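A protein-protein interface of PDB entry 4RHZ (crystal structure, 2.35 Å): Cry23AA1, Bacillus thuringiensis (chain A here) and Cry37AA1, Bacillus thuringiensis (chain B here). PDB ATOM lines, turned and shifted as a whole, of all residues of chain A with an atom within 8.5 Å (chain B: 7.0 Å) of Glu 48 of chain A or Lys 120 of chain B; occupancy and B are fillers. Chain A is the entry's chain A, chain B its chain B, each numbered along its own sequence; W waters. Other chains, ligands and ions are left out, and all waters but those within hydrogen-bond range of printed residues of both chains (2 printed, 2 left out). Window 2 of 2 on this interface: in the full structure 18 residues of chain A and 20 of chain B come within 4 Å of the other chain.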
ATOM      1  N   ILE A  45      10.898 -31.968   3.291  1.00  0.00           N
ATOM      2  CA  ILE A  45      10.653 -32.927   4.341  1.00  0.00           C
ATOM      3  C   ILE A  45       9.603 -32.290   5.220  1.00  0.00           C
ATOM      4  O   ILE A  45       9.801 -31.181   5.689  1.00  0.00           O
ATOM      5  CB  ILE A  45      11.908 -33.227   5.195  1.00  0.00           C
ATOM      6  CG1 ILE A  45      13.139 -33.586   4.322  1.00  0.00           C
ATOM      7  CG2 ILE A  45      11.606 -34.269   6.254  1.00  0.00           C
ATOM      8  CD1 ILE A  45      12.776 -34.514   3.181  1.00  0.00           C
ATOM      9  N   PRO A  46       8.492 -32.988   5.470  1.00  0.00           N
ATOM     10  CA  PRO A  46       7.486 -32.319   6.314  1.00  0.00           C
ATOM     11  C   PRO A  46       7.707 -32.501   7.814  1.00  0.00           C
ATOM     12  O   PRO A  46       6.795 -32.315   8.569  1.00  0.00           O
ATOM     13  CB  PRO A  46       6.160 -33.030   5.879  1.00  0.00           C
ATOM     14  CG  PRO A  46       6.635 -34.494   5.665  1.00  0.00           C
ATOM     15  CD  PRO A  46       8.088 -34.372   5.124  1.00  0.00           C
ATOM     16  N   THR A  47       8.864 -32.942   8.257  1.00  0.00           N
ATOM     17  CA  THR A  47       9.086 -33.111   9.683  1.00  0.00           C
ATOM     18  C   THR A  47      10.208 -32.111  10.031  1.00  0.00           C
ATOM     19  O   THR A  47      11.242 -32.044   9.322  1.00  0.00           O
ATOM     20  CB  THR A  47       9.496 -34.561   9.987  1.00  0.00           C
ATOM     21  OG1 THR A  47       8.333 -35.401   9.828  1.00  0.00           O
ATOM     22  CG2 THR A  47       9.948 -34.725  11.441  1.00  0.00           C
ATOM     23  N   GLU A  48      10.016 -31.306  11.067  1.00  0.00           N
ATOM     24  CA  GLU A  48      11.037 -30.273  11.349  1.00  0.00           C
ATOM     25  C   GLU A  48      12.349 -30.860  11.886  1.00  0.00           C
ATOM     26  O   GLU A  48      12.353 -31.877  12.590  1.00  0.00           O
ATOM     27  CB  GLU A  48      10.494 -29.238  12.346  1.00  0.00           C
ATOM     28  CG  GLU A  48       9.407 -28.266  11.803  1.00  0.00           C
ATOM     29  CD  GLU A  48       9.095 -27.143  12.834  1.00  0.00           C
ATOM     30  OE1 GLU A  48       9.738 -27.118  13.931  1.00  0.00           O
ATOM     31  OE2 GLU A  48       8.219 -26.295  12.544  1.00  0.00           O
ATOM     32  N   PRO A  49      13.469 -30.250  11.552  1.00  0.00           N
ATOM     33  CA  PRO A  49      14.682 -30.613  12.318  1.00  0.00           C
ATOM     34  C   PRO A  49      14.569 -30.430  13.854  1.00  0.00           C
ATOM     35  O   PRO A  49      13.762 -29.617  14.318  1.00  0.00           O
ATOM     36  CB  PRO A  49      15.762 -29.635  11.774  1.00  0.00           C
ATOM     37  CG  PRO A  49      15.200 -29.024  10.541  1.00  0.00           C
ATOM     38  CD  PRO A  49      13.706 -29.180  10.571  1.00  0.00           C
ATOM     39  N   VAL A  50      15.338 -31.211  14.608  1.00  0.00           N
ATOM     40  CA  VAL A  50      15.303 -31.196  16.020  1.00  0.00           C
ATOM     41  C   VAL A  50      16.710 -30.856  16.674  1.00  0.00           C
ATOM     42  O   VAL A  50      17.709 -31.563  16.429  1.00  0.00           O
ATOM     43  CB  VAL A  50      14.759 -32.554  16.611  1.00  0.00           C
ATOM     44  CG1 VAL A  50      14.820 -32.535  18.149  1.00  0.00           C
ATOM     45  CG2 VAL A  50      13.281 -32.805  16.145  1.00  0.00           C
ATOM     46  N   ASN A  51      16.714 -29.844  17.556  1.00  0.00           N
ATOM     47  CA  ASN A  51      17.882 -29.423  18.309  1.00  0.00           C
ATOM     48  C   ASN A  51      17.932 -30.282  19.518  1.00  0.00           C
ATOM     49  O   ASN A  51      16.989 -30.314  20.274  1.00  0.00           O
ATOM     50  CB  ASN A  51      17.775 -27.925  18.734  1.00  0.00           C
ATOM     51  CG  ASN A  51      18.133 -26.955  17.574  1.00  0.00           C
ATOM     52  OD1 ASN A  51      18.592 -27.385  16.466  1.00  0.00           O
ATOM     53  ND2 ASN A  51      17.970 -25.634  17.823  1.00  0.00           N
ATOM     54  N   GLY A 104      14.722 -29.927   1.230  1.00  0.00           N
ATOM     55  CA  GLY A 104      14.555 -28.859   2.219  1.00  0.00           C
ATOM     56  C   GLY A 104      13.698 -29.340   3.375  1.00  0.00           C
ATOM     57  O   GLY A 104      13.167 -30.457   3.354  1.00  0.00           O
ATOM     58  N   PHE A 105      13.547 -28.506   4.387  1.00  0.00           N
ATOM     59  CA  PHE A 105      12.651 -28.814   5.512  1.00  0.00           C
ATOM     60  C   PHE A 105      11.563 -27.749   5.663  1.00  0.00           C
ATOM     61  O   PHE A 105      11.871 -26.573   5.590  1.00  0.00           O
ATOM     62  CB  PHE A 105      13.461 -28.926   6.789  1.00  0.00           C
ATOM     63  CG  PHE A 105      14.373 -30.097   6.810  1.00  0.00           C
ATOM     64  CD1 PHE A 105      15.609 -30.038   6.202  1.00  0.00           C
ATOM     65  CD2 PHE A 105      13.989 -31.266   7.433  1.00  0.00           C
ATOM     66  CE1 PHE A 105      16.435 -31.128   6.211  1.00  0.00           C
ATOM     67  CE2 PHE A 105      14.822 -32.333   7.470  1.00  0.00           C
ATOM     68  CZ  PHE A 105      16.044 -32.276   6.859  1.00  0.00           C
ATOM     69  N   VAL A 106      10.305 -28.155   5.850  1.00  0.00           N
ATOM     70  CA  VAL A 106       9.215 -27.183   5.886  1.00  0.00           C
ATOM     71  C   VAL A 106       9.392 -26.255   7.083  1.00  0.00           C
ATOM     72  O   VAL A 106       9.800 -26.666   8.188  1.00  0.00           O
ATOM     73  CB  VAL A 106       7.740 -27.778   5.896  1.00  0.00           C
ATOM     74  CG1 VAL A 106       7.275 -28.365   4.479  1.00  0.00           C
ATOM     75  CG2 VAL A 106       7.524 -28.748   7.062  1.00  0.00           C
ATOM     76  N   ASN A 107       9.072 -24.999   6.813  1.00  0.00           N
ATOM     77  CA  ASN A 107       9.180 -23.893   7.768  1.00  0.00           C
ATOM     78  C   ASN A 107      10.632 -23.418   7.972  1.00  0.00           C
ATOM     79  O   ASN A 107      10.848 -22.509   8.789  1.00  0.00           O
ATOM     80  CB  ASN A 107       8.442 -24.174   9.114  1.00  0.00           C
ATOM     81  CG  ASN A 107       6.979 -24.733   8.930  1.00  0.00           C
ATOM     82  OD1 ASN A 107       6.212 -24.253   8.073  1.00  0.00           O
ATOM     83  ND2 ASN A 107       6.601 -25.738   9.759  1.00  0.00           N
ATOM     84  N   SER A 108      11.614 -23.976   7.247  1.00  0.00           N
ATOM     85  CA  SER A 108      13.009 -23.463   7.365  1.00  0.00           C
ATOM     86  C   SER A 108      13.904 -23.458   6.125  1.00  0.00           C
ATOM     87  O   SER A 108      13.428 -23.474   4.992  1.00  0.00           O
ATOM     88  CB  SER A 108      13.769 -24.071   8.539  1.00  0.00           C
ATOM     89  OG  SER A 108      13.780 -25.478   8.479  1.00  0.00           O
ATOM     90  N   VAL A 110      17.341 -24.788   5.572  1.00  0.00           N
ATOM     91  CA  VAL A 110      18.472 -25.637   5.416  1.00  0.00           C
ATOM     92  C   VAL A 110      18.083 -26.657   4.306  1.00  0.00           C
ATOM     93  O   VAL A 110      16.897 -26.985   4.132  1.00  0.00           O
ATOM     94  CB  VAL A 110      18.838 -26.175   6.814  1.00  0.00           C
ATOM     95  CG1 VAL A 110      17.580 -26.129   7.728  1.00  0.00           C
ATOM     96  CG2 VAL A 110      19.504 -27.533   6.771  1.00  0.00           C
ATOM     97  N   GLN A 155      21.700 -30.301  15.613  1.00  0.00           N
ATOM     98  CA  GLN A 155      20.451 -30.221  14.954  1.00  0.00           C
ATOM     99  C   GLN A 155      20.296 -31.441  13.989  1.00  0.00           C
ATOM    100  O   GLN A 155      20.966 -31.518  12.973  1.00  0.00           O
ATOM    101  CB  GLN A 155      20.333 -28.899  14.211  1.00  0.00           C
ATOM    102  CG  GLN A 155      19.038 -28.713  13.571  1.00  0.00           C
ATOM    103  CD  GLN A 155      18.852 -27.342  13.029  1.00  0.00           C
ATOM    104  OE1 GLN A 155      18.808 -27.139  11.809  1.00  0.00           O
ATOM    105  NE2 GLN A 155      18.749 -26.351  13.941  1.00  0.00           N
ATOM    106  N   ASN A 156      19.398 -32.345  14.352  1.00  0.00           N
ATOM    107  CA  ASN A 156      19.082 -33.570  13.621  1.00  0.00           C
ATOM    108  C   ASN A 156      17.960 -33.446  12.646  1.00  0.00           C
ATOM    109  O   ASN A 156      16.946 -32.809  12.951  1.00  0.00           O
ATOM    110  CB  ASN A 156      18.719 -34.672  14.595  1.00  0.00           C
ATOM    111  CG  ASN A 156      19.810 -35.651  14.702  1.00  0.00           C
ATOM    112  OD1 ASN A 156      20.822 -35.432  15.441  1.00  0.00           O
ATOM    113  ND2 ASN A 156      19.701 -36.750  13.880  1.00  0.00           N
ATOM    114  N   GLY A 157      18.147 -34.044  11.473  1.00  0.00           N
ATOM    115  CA  GLY A 157      17.050 -34.199  10.478  1.00  0.00           C
ATOM    116  C   GLY A 157      16.848 -35.670  10.082  1.00  0.00           C
ATOM    117  O   GLY A 157      17.813 -36.431  10.057  1.00  0.00           O
ATOM    118  N   THR A 158      15.595 -36.061   9.861  1.00  0.00           N
ATOM    119  CA  THR A 158      15.280 -37.397   9.347  1.00  0.00           C
ATOM    120  C   THR A 158      14.329 -37.279   8.190  1.00  0.00           C
ATOM    121  O   THR A 158      13.471 -36.373   8.137  1.00  0.00           O
ATOM    122  CB  THR A 158      14.540 -38.264  10.313  1.00  0.00           C
ATOM    123  OG1 THR A 158      13.317 -37.599  10.650  1.00  0.00           O
ATOM    124  CG2 THR A 158      15.382 -38.553  11.543  1.00  0.00           C
ATOM    125  N   LEU A 225      22.496 -32.215  11.015  1.00  0.00           N
ATOM    126  CA  LEU A 225      22.569 -31.231   9.975  1.00  0.00           C
ATOM    127  C   LEU A 225      23.513 -30.089  10.265  1.00  0.00           C
ATOM    128  O   LEU A 225      24.092 -29.535   9.331  1.00  0.00           O
ATOM    129  CB  LEU A 225      21.217 -30.630   9.714  1.00  0.00           C
ATOM    130  CG  LEU A 225      20.059 -31.572   9.427  1.00  0.00           C
ATOM    131  CD1 LEU A 225      18.789 -30.719   9.553  1.00  0.00           C
ATOM    132  CD2 LEU A 225      20.196 -32.171   7.968  1.00  0.00           C
ATOM    133  N   THR B   7       2.581 -19.656  18.158  1.00  0.00           N
ATOM    134  CA  THR B   7       1.815 -20.903  18.322  1.00  0.00           C
ATOM    135  C   THR B   7       2.806 -22.022  18.593  1.00  0.00           C
ATOM    136  O   THR B   7       3.700 -22.261  17.826  1.00  0.00           O
ATOM    137  CB  THR B   7       0.913 -21.208  17.048  1.00  0.00           C
ATOM    138  OG1 THR B   7      -0.012 -20.114  16.822  1.00  0.00           O
ATOM    139  CG2 THR B   7       0.089 -22.595  17.180  1.00  0.00           C
ATOM    140  N   PHE B   8       2.657 -22.642  19.755  1.00  0.00           N
ATOM    141  CA  PHE B   8       3.552 -23.590  20.299  1.00  0.00           C
ATOM    142  C   PHE B   8       2.873 -24.915  20.177  1.00  0.00           C
ATOM    143  O   PHE B   8       1.699 -25.040  20.551  1.00  0.00           O
ATOM    144  CB  PHE B   8       3.799 -23.254  21.809  1.00  0.00           C
ATOM    145  CG  PHE B   8       4.461 -21.903  21.994  1.00  0.00           C
ATOM    146  CD1 PHE B   8       3.697 -20.761  22.277  1.00  0.00           C
ATOM    147  CD2 PHE B   8       5.819 -21.749  21.756  1.00  0.00           C
ATOM    148  CE1 PHE B   8       4.283 -19.525  22.368  1.00  0.00           C
ATOM    149  CE2 PHE B   8       6.436 -20.502  21.848  1.00  0.00           C
ATOM    150  CZ  PHE B   8       5.672 -19.389  22.167  1.00  0.00           C
ATOM    151  N   THR B   9       3.601 -25.924  19.684  1.00  0.00           N
ATOM    152  CA  THR B   9       2.995 -27.271  19.667  1.00  0.00           C
ATOM    153  C   THR B   9       3.879 -28.159  20.447  1.00  0.00           C
ATOM    154  O   THR B   9       4.993 -28.371  20.059  1.00  0.00           O
ATOM    155  CB  THR B   9       2.886 -27.824  18.236  1.00  0.00           C
ATOM    156  OG1 THR B   9       2.141 -26.891  17.474  1.00  0.00           O
ATOM    157  CG2 THR B   9       2.170 -29.173  18.233  1.00  0.00           C
ATOM    158  N   ILE B  10       3.366 -28.707  21.520  1.00  0.00           N
ATOM    159  CA  ILE B  10       4.167 -29.408  22.410  1.00  0.00           C
ATOM    160  C   ILE B  10       3.737 -30.866  22.420  1.00  0.00           C
ATOM    161  O   ILE B  10       2.521 -31.145  22.507  1.00  0.00           O
ATOM    162  CB  ILE B  10       3.912 -28.850  23.836  1.00  0.00           C
ATOM    163  CG1 ILE B  10       4.150 -27.306  23.881  1.00  0.00           C
ATOM    164  CG2 ILE B  10       4.678 -29.630  24.838  1.00  0.00           C
ATOM    165  CD1 ILE B  10       3.877 -26.695  25.240  1.00  0.00           C
ATOM    166  N   ASN B  11       4.727 -31.792  22.388  1.00  0.00           N
ATOM    167  CA  ASN B  11       4.454 -33.208  22.473  1.00  0.00           C
ATOM    168  C   ASN B  11       5.160 -33.846  23.603  1.00  0.00           C
ATOM    169  O   ASN B  11       6.352 -33.589  23.795  1.00  0.00           O
ATOM    170  CB  ASN B  11       4.877 -33.865  21.172  1.00  0.00           C
ATOM    171  CG  ASN B  11       3.811 -33.737  20.131  1.00  0.00           C
ATOM    172  OD1 ASN B  11       2.820 -34.424  20.219  1.00  0.00           O
ATOM    173  ND2 ASN B  11       3.962 -32.818  19.186  1.00  0.00           N
ATOM    174  N   ILE B  40       4.238 -21.496  28.558  1.00  0.00           N
ATOM    175  CA  ILE B  40       3.495 -21.950  27.389  1.00  0.00           C
ATOM    176  C   ILE B  40       2.662 -23.196  27.714  1.00  0.00           C
ATOM    177  O   ILE B  40       1.812 -23.600  26.932  1.00  0.00           O
ATOM    178  CB  ILE B  40       4.436 -22.131  26.140  1.00  0.00           C
ATOM    179  CG1 ILE B  40       5.374 -23.340  26.306  1.00  0.00           C
ATOM    180  CG2 ILE B  40       5.195 -20.814  25.913  1.00  0.00           C
ATOM    181  CD1 ILE B  40       6.122 -23.803  24.996  1.00  0.00           C
ATOM    182  N   PHE B  75      13.743 -22.704  25.550  1.00  0.00           N
ATOM    183  CA  PHE B  75      12.638 -23.377  26.239  1.00  0.00           C
ATOM    184  C   PHE B  75      13.203 -24.202  27.355  1.00  0.00           C
ATOM    185  O   PHE B  75      14.324 -24.724  27.232  1.00  0.00           O
ATOM    186  CB  PHE B  75      11.882 -24.321  25.280  1.00  0.00           C
ATOM    187  CG  PHE B  75      11.255 -23.651  24.099  1.00  0.00           C
ATOM    188  CD1 PHE B  75      11.940 -23.566  22.888  1.00  0.00           C
ATOM    189  CD2 PHE B  75       9.961 -23.152  24.169  1.00  0.00           C
ATOM    190  CE1 PHE B  75      11.366 -22.927  21.765  1.00  0.00           C
ATOM    191  CE2 PHE B  75       9.316 -22.558  23.019  1.00  0.00           C
ATOM    192  CZ  PHE B  75      10.026 -22.401  21.835  1.00  0.00           C
ATOM    193  N   SER B 100      15.849 -22.608  19.658  1.00  0.00           N
ATOM    194  CA  SER B 100      15.876 -22.791  18.217  1.00  0.00           C
ATOM    195  C   SER B 100      15.307 -21.560  17.503  1.00  0.00           C
ATOM    196  O   SER B 100      14.609 -20.765  18.106  1.00  0.00           O
ATOM    197  CB  SER B 100      14.975 -23.989  17.856  1.00  0.00           C
ATOM    198  OG  SER B 100      13.667 -23.758  18.372  1.00  0.00           O
ATOM    199  N   THR B 101      15.568 -21.442  16.211  1.00  0.00           N
ATOM    200  CA  THR B 101      14.806 -20.562  15.322  1.00  0.00           C
ATOM    201  C   THR B 101      13.393 -21.137  14.996  1.00  0.00           C
ATOM    202  O   THR B 101      13.187 -22.327  15.108  1.00  0.00           O
ATOM    203  CB  THR B 101      15.536 -20.478  13.986  1.00  0.00           C
ATOM    204  OG1 THR B 101      15.665 -21.822  13.480  1.00  0.00           O
ATOM    205  CG2 THR B 101      16.965 -19.870  14.168  1.00  0.00           C
ATOM    206  N   PRO B 102      12.411 -20.287  14.612  1.00  0.00           N
ATOM    207  CA  PRO B 102      11.076 -20.850  14.312  1.00  0.00           C
ATOM    208  C   PRO B 102      11.170 -21.784  13.097  1.00  0.00           C
ATOM    209  O   PRO B 102      11.823 -21.443  12.131  1.00  0.00           O
ATOM    210  CB  PRO B 102      10.226 -19.606  13.960  1.00  0.00           C
ATOM    211  CG  PRO B 102      11.214 -18.565  13.552  1.00  0.00           C
ATOM    212  CD  PRO B 102      12.491 -18.837  14.293  1.00  0.00           C
ATOM    213  N   GLY B 103      10.588 -22.973  13.187  1.00  0.00           N
ATOM    214  CA  GLY B 103      10.750 -23.928  12.077  1.00  0.00           C
ATOM    215  C   GLY B 103      11.689 -25.024  12.497  1.00  0.00           C
ATOM    216  O   GLY B 103      11.756 -26.066  11.816  1.00  0.00           O
ATOM    217  N   VAL B 104      12.446 -24.812  13.590  1.00  0.00           N
ATOM    218  CA  VAL B 104      13.234 -25.893  14.148  1.00  0.00           C
ATOM    219  C   VAL B 104      12.617 -26.216  15.476  1.00  0.00           C
ATOM    220  O   VAL B 104      12.148 -25.278  16.206  1.00  0.00           O
ATOM    221  CB  VAL B 104      14.680 -25.519  14.311  1.00  0.00           C
ATOM    222  CG1 VAL B 104      15.475 -26.602  15.055  1.00  0.00           C
ATOM    223  CG2 VAL B 104      15.350 -25.175  12.932  1.00  0.00           C
ATOM    224  N   THR B 105      12.550 -27.520  15.781  1.00  0.00           N
ATOM    225  CA  THR B 105      11.872 -28.001  16.950  1.00  0.00           C
ATOM    226  C   THR B 105      12.942 -28.303  17.993  1.00  0.00           C
ATOM    227  O   THR B 105      14.065 -28.672  17.624  1.00  0.00           O
ATOM    228  CB  THR B 105      11.066 -29.257  16.558  1.00  0.00           C
ATOM    229  OG1 THR B 105       9.872 -28.823  15.899  1.00  0.00           O
ATOM    230  CG2 THR B 105      10.678 -30.121  17.711  1.00  0.00           C
ATOM    231  N   VAL B 106      12.624 -28.167  19.287  1.00  0.00           N
ATOM    232  CA  VAL B 106      13.588 -28.564  20.298  1.00  0.00           C
ATOM    233  C   VAL B 106      13.085 -29.760  21.091  1.00  0.00           C
ATOM    234  O   VAL B 106      11.889 -29.900  21.287  1.00  0.00           O
ATOM    235  CB  VAL B 106      13.945 -27.386  21.386  1.00  0.00           C
ATOM    236  CG1 VAL B 106      14.395 -26.100  20.762  1.00  0.00           C
ATOM    237  CG2 VAL B 106      12.795 -27.179  22.384  1.00  0.00           C
ATOM    238  N   THR B 118       8.938 -32.393  23.188  1.00  0.00           N
ATOM    239  CA  THR B 118       9.418 -31.632  22.091  1.00  0.00           C
ATOM    240  C   THR B 118       8.542 -30.367  21.910  1.00  0.00           C
ATOM    241  O   THR B 118       7.367 -30.352  22.310  1.00  0.00           O
ATOM    242  CB  THR B 118       9.400 -32.419  20.762  1.00  0.00           C
ATOM    243  OG1 THR B 118       8.056 -32.600  20.307  1.00  0.00           O
ATOM    244  CG2 THR B 118      10.190 -33.756  20.796  1.00  0.00           C
ATOM    245  N   ILE B 119       9.093 -29.284  21.333  1.00  0.00           N
ATOM    246  CA  ILE B 119       8.326 -28.084  21.179  1.00  0.00           C
ATOM    247  C   ILE B 119       8.635 -27.506  19.849  1.00  0.00           C
ATOM    248  O   ILE B 119       9.794 -27.348  19.471  1.00  0.00           O
ATOM    249  CB  ILE B 119       8.712 -26.984  22.265  1.00  0.00           C
ATOM    250  CG1 ILE B 119       8.313 -27.405  23.660  1.00  0.00           C
ATOM    251  CG2 ILE B 119       7.894 -25.695  22.092  1.00  0.00           C
ATOM    252  CD1 ILE B 119       9.378 -27.897  24.408  1.00  0.00           C
ATOM    253  N   LYS B 120       7.598 -27.112  19.145  1.00  0.00           N
ATOM    254  CA  LYS B 120       7.721 -26.531  17.827  1.00  0.00           C
ATOM    255  C   LYS B 120       7.006 -25.222  17.931  1.00  0.00           C
ATOM    256  O   LYS B 120       6.061 -25.163  18.689  1.00  0.00           O
ATOM    257  CB  LYS B 120       6.889 -27.440  16.932  1.00  0.00           C
ATOM    258  CG  LYS B 120       6.501 -26.880  15.647  1.00  0.00           C
ATOM    259  CD  LYS B 120       5.408 -27.748  14.992  1.00  0.00           C
ATOM    260  CE  LYS B 120       5.145 -27.220  13.584  1.00  0.00           C
ATOM    261  NZ  LYS B 120       3.936 -27.885  12.994  1.00  0.00           N
ATOM    262  N   TYR B 121       7.430 -24.172  17.220  1.00  0.00           N
ATOM    263  CA  TYR B 121       6.702 -22.929  17.317  1.00  0.00           C
ATOM    264  C   TYR B 121       6.721 -22.229  16.005  1.00  0.00           C
ATOM    265  O   TYR B 121       7.635 -22.458  15.250  1.00  0.00           O
ATOM    266  CB  TYR B 121       7.288 -21.998  18.416  1.00  0.00           C
ATOM    267  CG  TYR B 121       8.634 -21.344  18.145  1.00  0.00           C
ATOM    268  CD1 TYR B 121       8.712 -19.993  17.815  1.00  0.00           C
ATOM    269  CD2 TYR B 121       9.829 -22.067  18.263  1.00  0.00           C
ATOM    270  CE1 TYR B 121       9.945 -19.363  17.587  1.00  0.00           C
ATOM    271  CE2 TYR B 121      11.092 -21.423  18.094  1.00  0.00           C
ATOM    272  CZ  TYR B 121      11.130 -20.077  17.755  1.00  0.00           C
ATOM    273  OH  TYR B 121      12.367 -19.467  17.531  1.00  0.00           O
ATOM    274  N   SER B 122       5.729 -21.362  15.770  1.00  0.00           N
ATOM    275  CA  SER B 122       5.683 -20.530  14.575  1.00  0.00           C
ATOM    276  C   SER B 122       5.079 -19.176  14.919  1.00  0.00           C
ATOM    277  O   SER B 122       4.370 -19.038  15.925  1.00  0.00           O
ATOM    278  CB  SER B 122       4.826 -21.190  13.460  1.00  0.00           C
ATOM    279  OG  SER B 122       3.501 -21.447  13.904  1.00  0.00           O
HETATM  280  O   HOH W   1       9.658 -24.679  15.543  1.00  0.00           O
HETATM  281  O   HOH W   2       7.112 -24.062  13.077  1.00  0.00           O
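C of Val 104 of chain B touches OE1 of Glu 48 of chain A, 3.4 Å away. OE2 of Glu 48 of chain A touches CE of Lys 120 of chain B, at 3.4 Å. CD of Pro 49 of chain A touches O of Gly 103 of chain B, at 3.9 Å. Pro 49 of chain A touches Val 104 of chain B (O to CG1, 3.5 Å). Asn 51 of chain A touches Ser 100 of chain B. OD1 of Asn 51 of chain A touches CG1 of Val 104 of chain B, at 3.5 Å. Val 106 of chain B touches Asn 51 of chain A (CA to O, 3.8 Å). O of Asn 107 of chain A touches O of Pro 102 of chain B, 3.6 Å away. Asn 107 of chain A touches Gly 103 of chain B (O to CA, 3.6 Å). Gln 155 of chain A touches Val 104 of chain B (NE2 to CG1, 3.5 Å).
Water W2 bridges the side-chain carboxylate (OE2) of Glu 48 of chain A (2.5 Å) and the backbone carbonyl oxygen (O) of Tyr 121 of chain B (2.8 Å). Water W1 lies within hydrogen-bond range of the backbone carbonyl oxygen (O) of Val 104 of chain B (2.6 Å), the backbone NH (N) of Tyr 121 of chain B (2.8 Å), the side-chain carboxylate (OE1) of Glu 48 of chain A (2.9 Å) and the backbone NH (N) of Gly 103 of chain B (3.1 Å).
The side-chain carboxylate (OE1) of Glu 48 of chain A is in hydrogen-bond range of the side-chain hydroxyl (OG1) of Thr 105 of chain B (2.6 Å). The backbone carbonyl oxygen (O) of Pro 49 of chain A lies within hydrogen-bond range of the backbone NH (N) of Thr 105 of chain B (2.8 Å). The backbone NH of Asn 51 of chain A is in hydrogen-bond range of the backbone carbonyl oxygen of Thr 105 of chain B, at 2.9 Å. O of Gly 103 of chain B sits close to OE1 of Glu 48 of chain A (3.1 Å).
Of the 18 printed residues of chain A, 7 touch a printed residue of chain B. Hydrophobic or aromatic side chains of chain A that line the printed part of chain B: Pro 49 and Val 50. Among the printed residues, no Asp or Glu carboxylate lies within 4 Å of a Lys or Arg side-chain nitrogen of the other chain.
The side-chain carboxylate of Glu 48 of chain A sits at hydrogen-bond distance from the side-chain amide nitrogen of Asn 107 of chain A, at 3.3 Å. O of Val 50 of chain A is in hydrogen-bond range of N of Asn 156 of chain A, at 2.8 Å. The side-chain amide oxygen (OD1) of Asn 51 of chain A is in hydrogen-bond range of the side-chain amide nitrogen (NE2) of Gln 155 of chain A, at 2.7 Å. N of Leu 225 of chain A sits at hydrogen-bond distance from O of Gln 155 of chain A (2.6 Å). O of Ser 100 of chain B sits at hydrogen-bond distance from OH of Tyr 121 of chain B (2.7 Å). O of Val 106 of chain B sits at hydrogen-bond distance from N of Ile 119 of chain B, 2.9 Å away.
Of chain B, only Gly 103 (3.0 Å), Val 104 (3.4 Å), Thr 105 (2.6 Å) and Lys 120 (3.4 Å) come within 4 Å of Glu 48 of chain A. Of the printed residues of chain A, Ser 100 of chain B touches Asn 51. Of the printed residues of chain A, Val 104 of chain B touches Glu 48, Pro 49, Asn 51 and Gln 155. Printed residues of chain A within 4 Å of Val 106 of chain B: Asn 51. Lys 120 of chain B touches one residue of chain A. The nearest residue of chain B that does not touch Glu 48 of chain A is Tyr 121 of chain B (4.7 Å). The nearest printed residue of chain B that does not touch Asn 51 of chain A is Thr 101 of chain B (5.1 Å).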
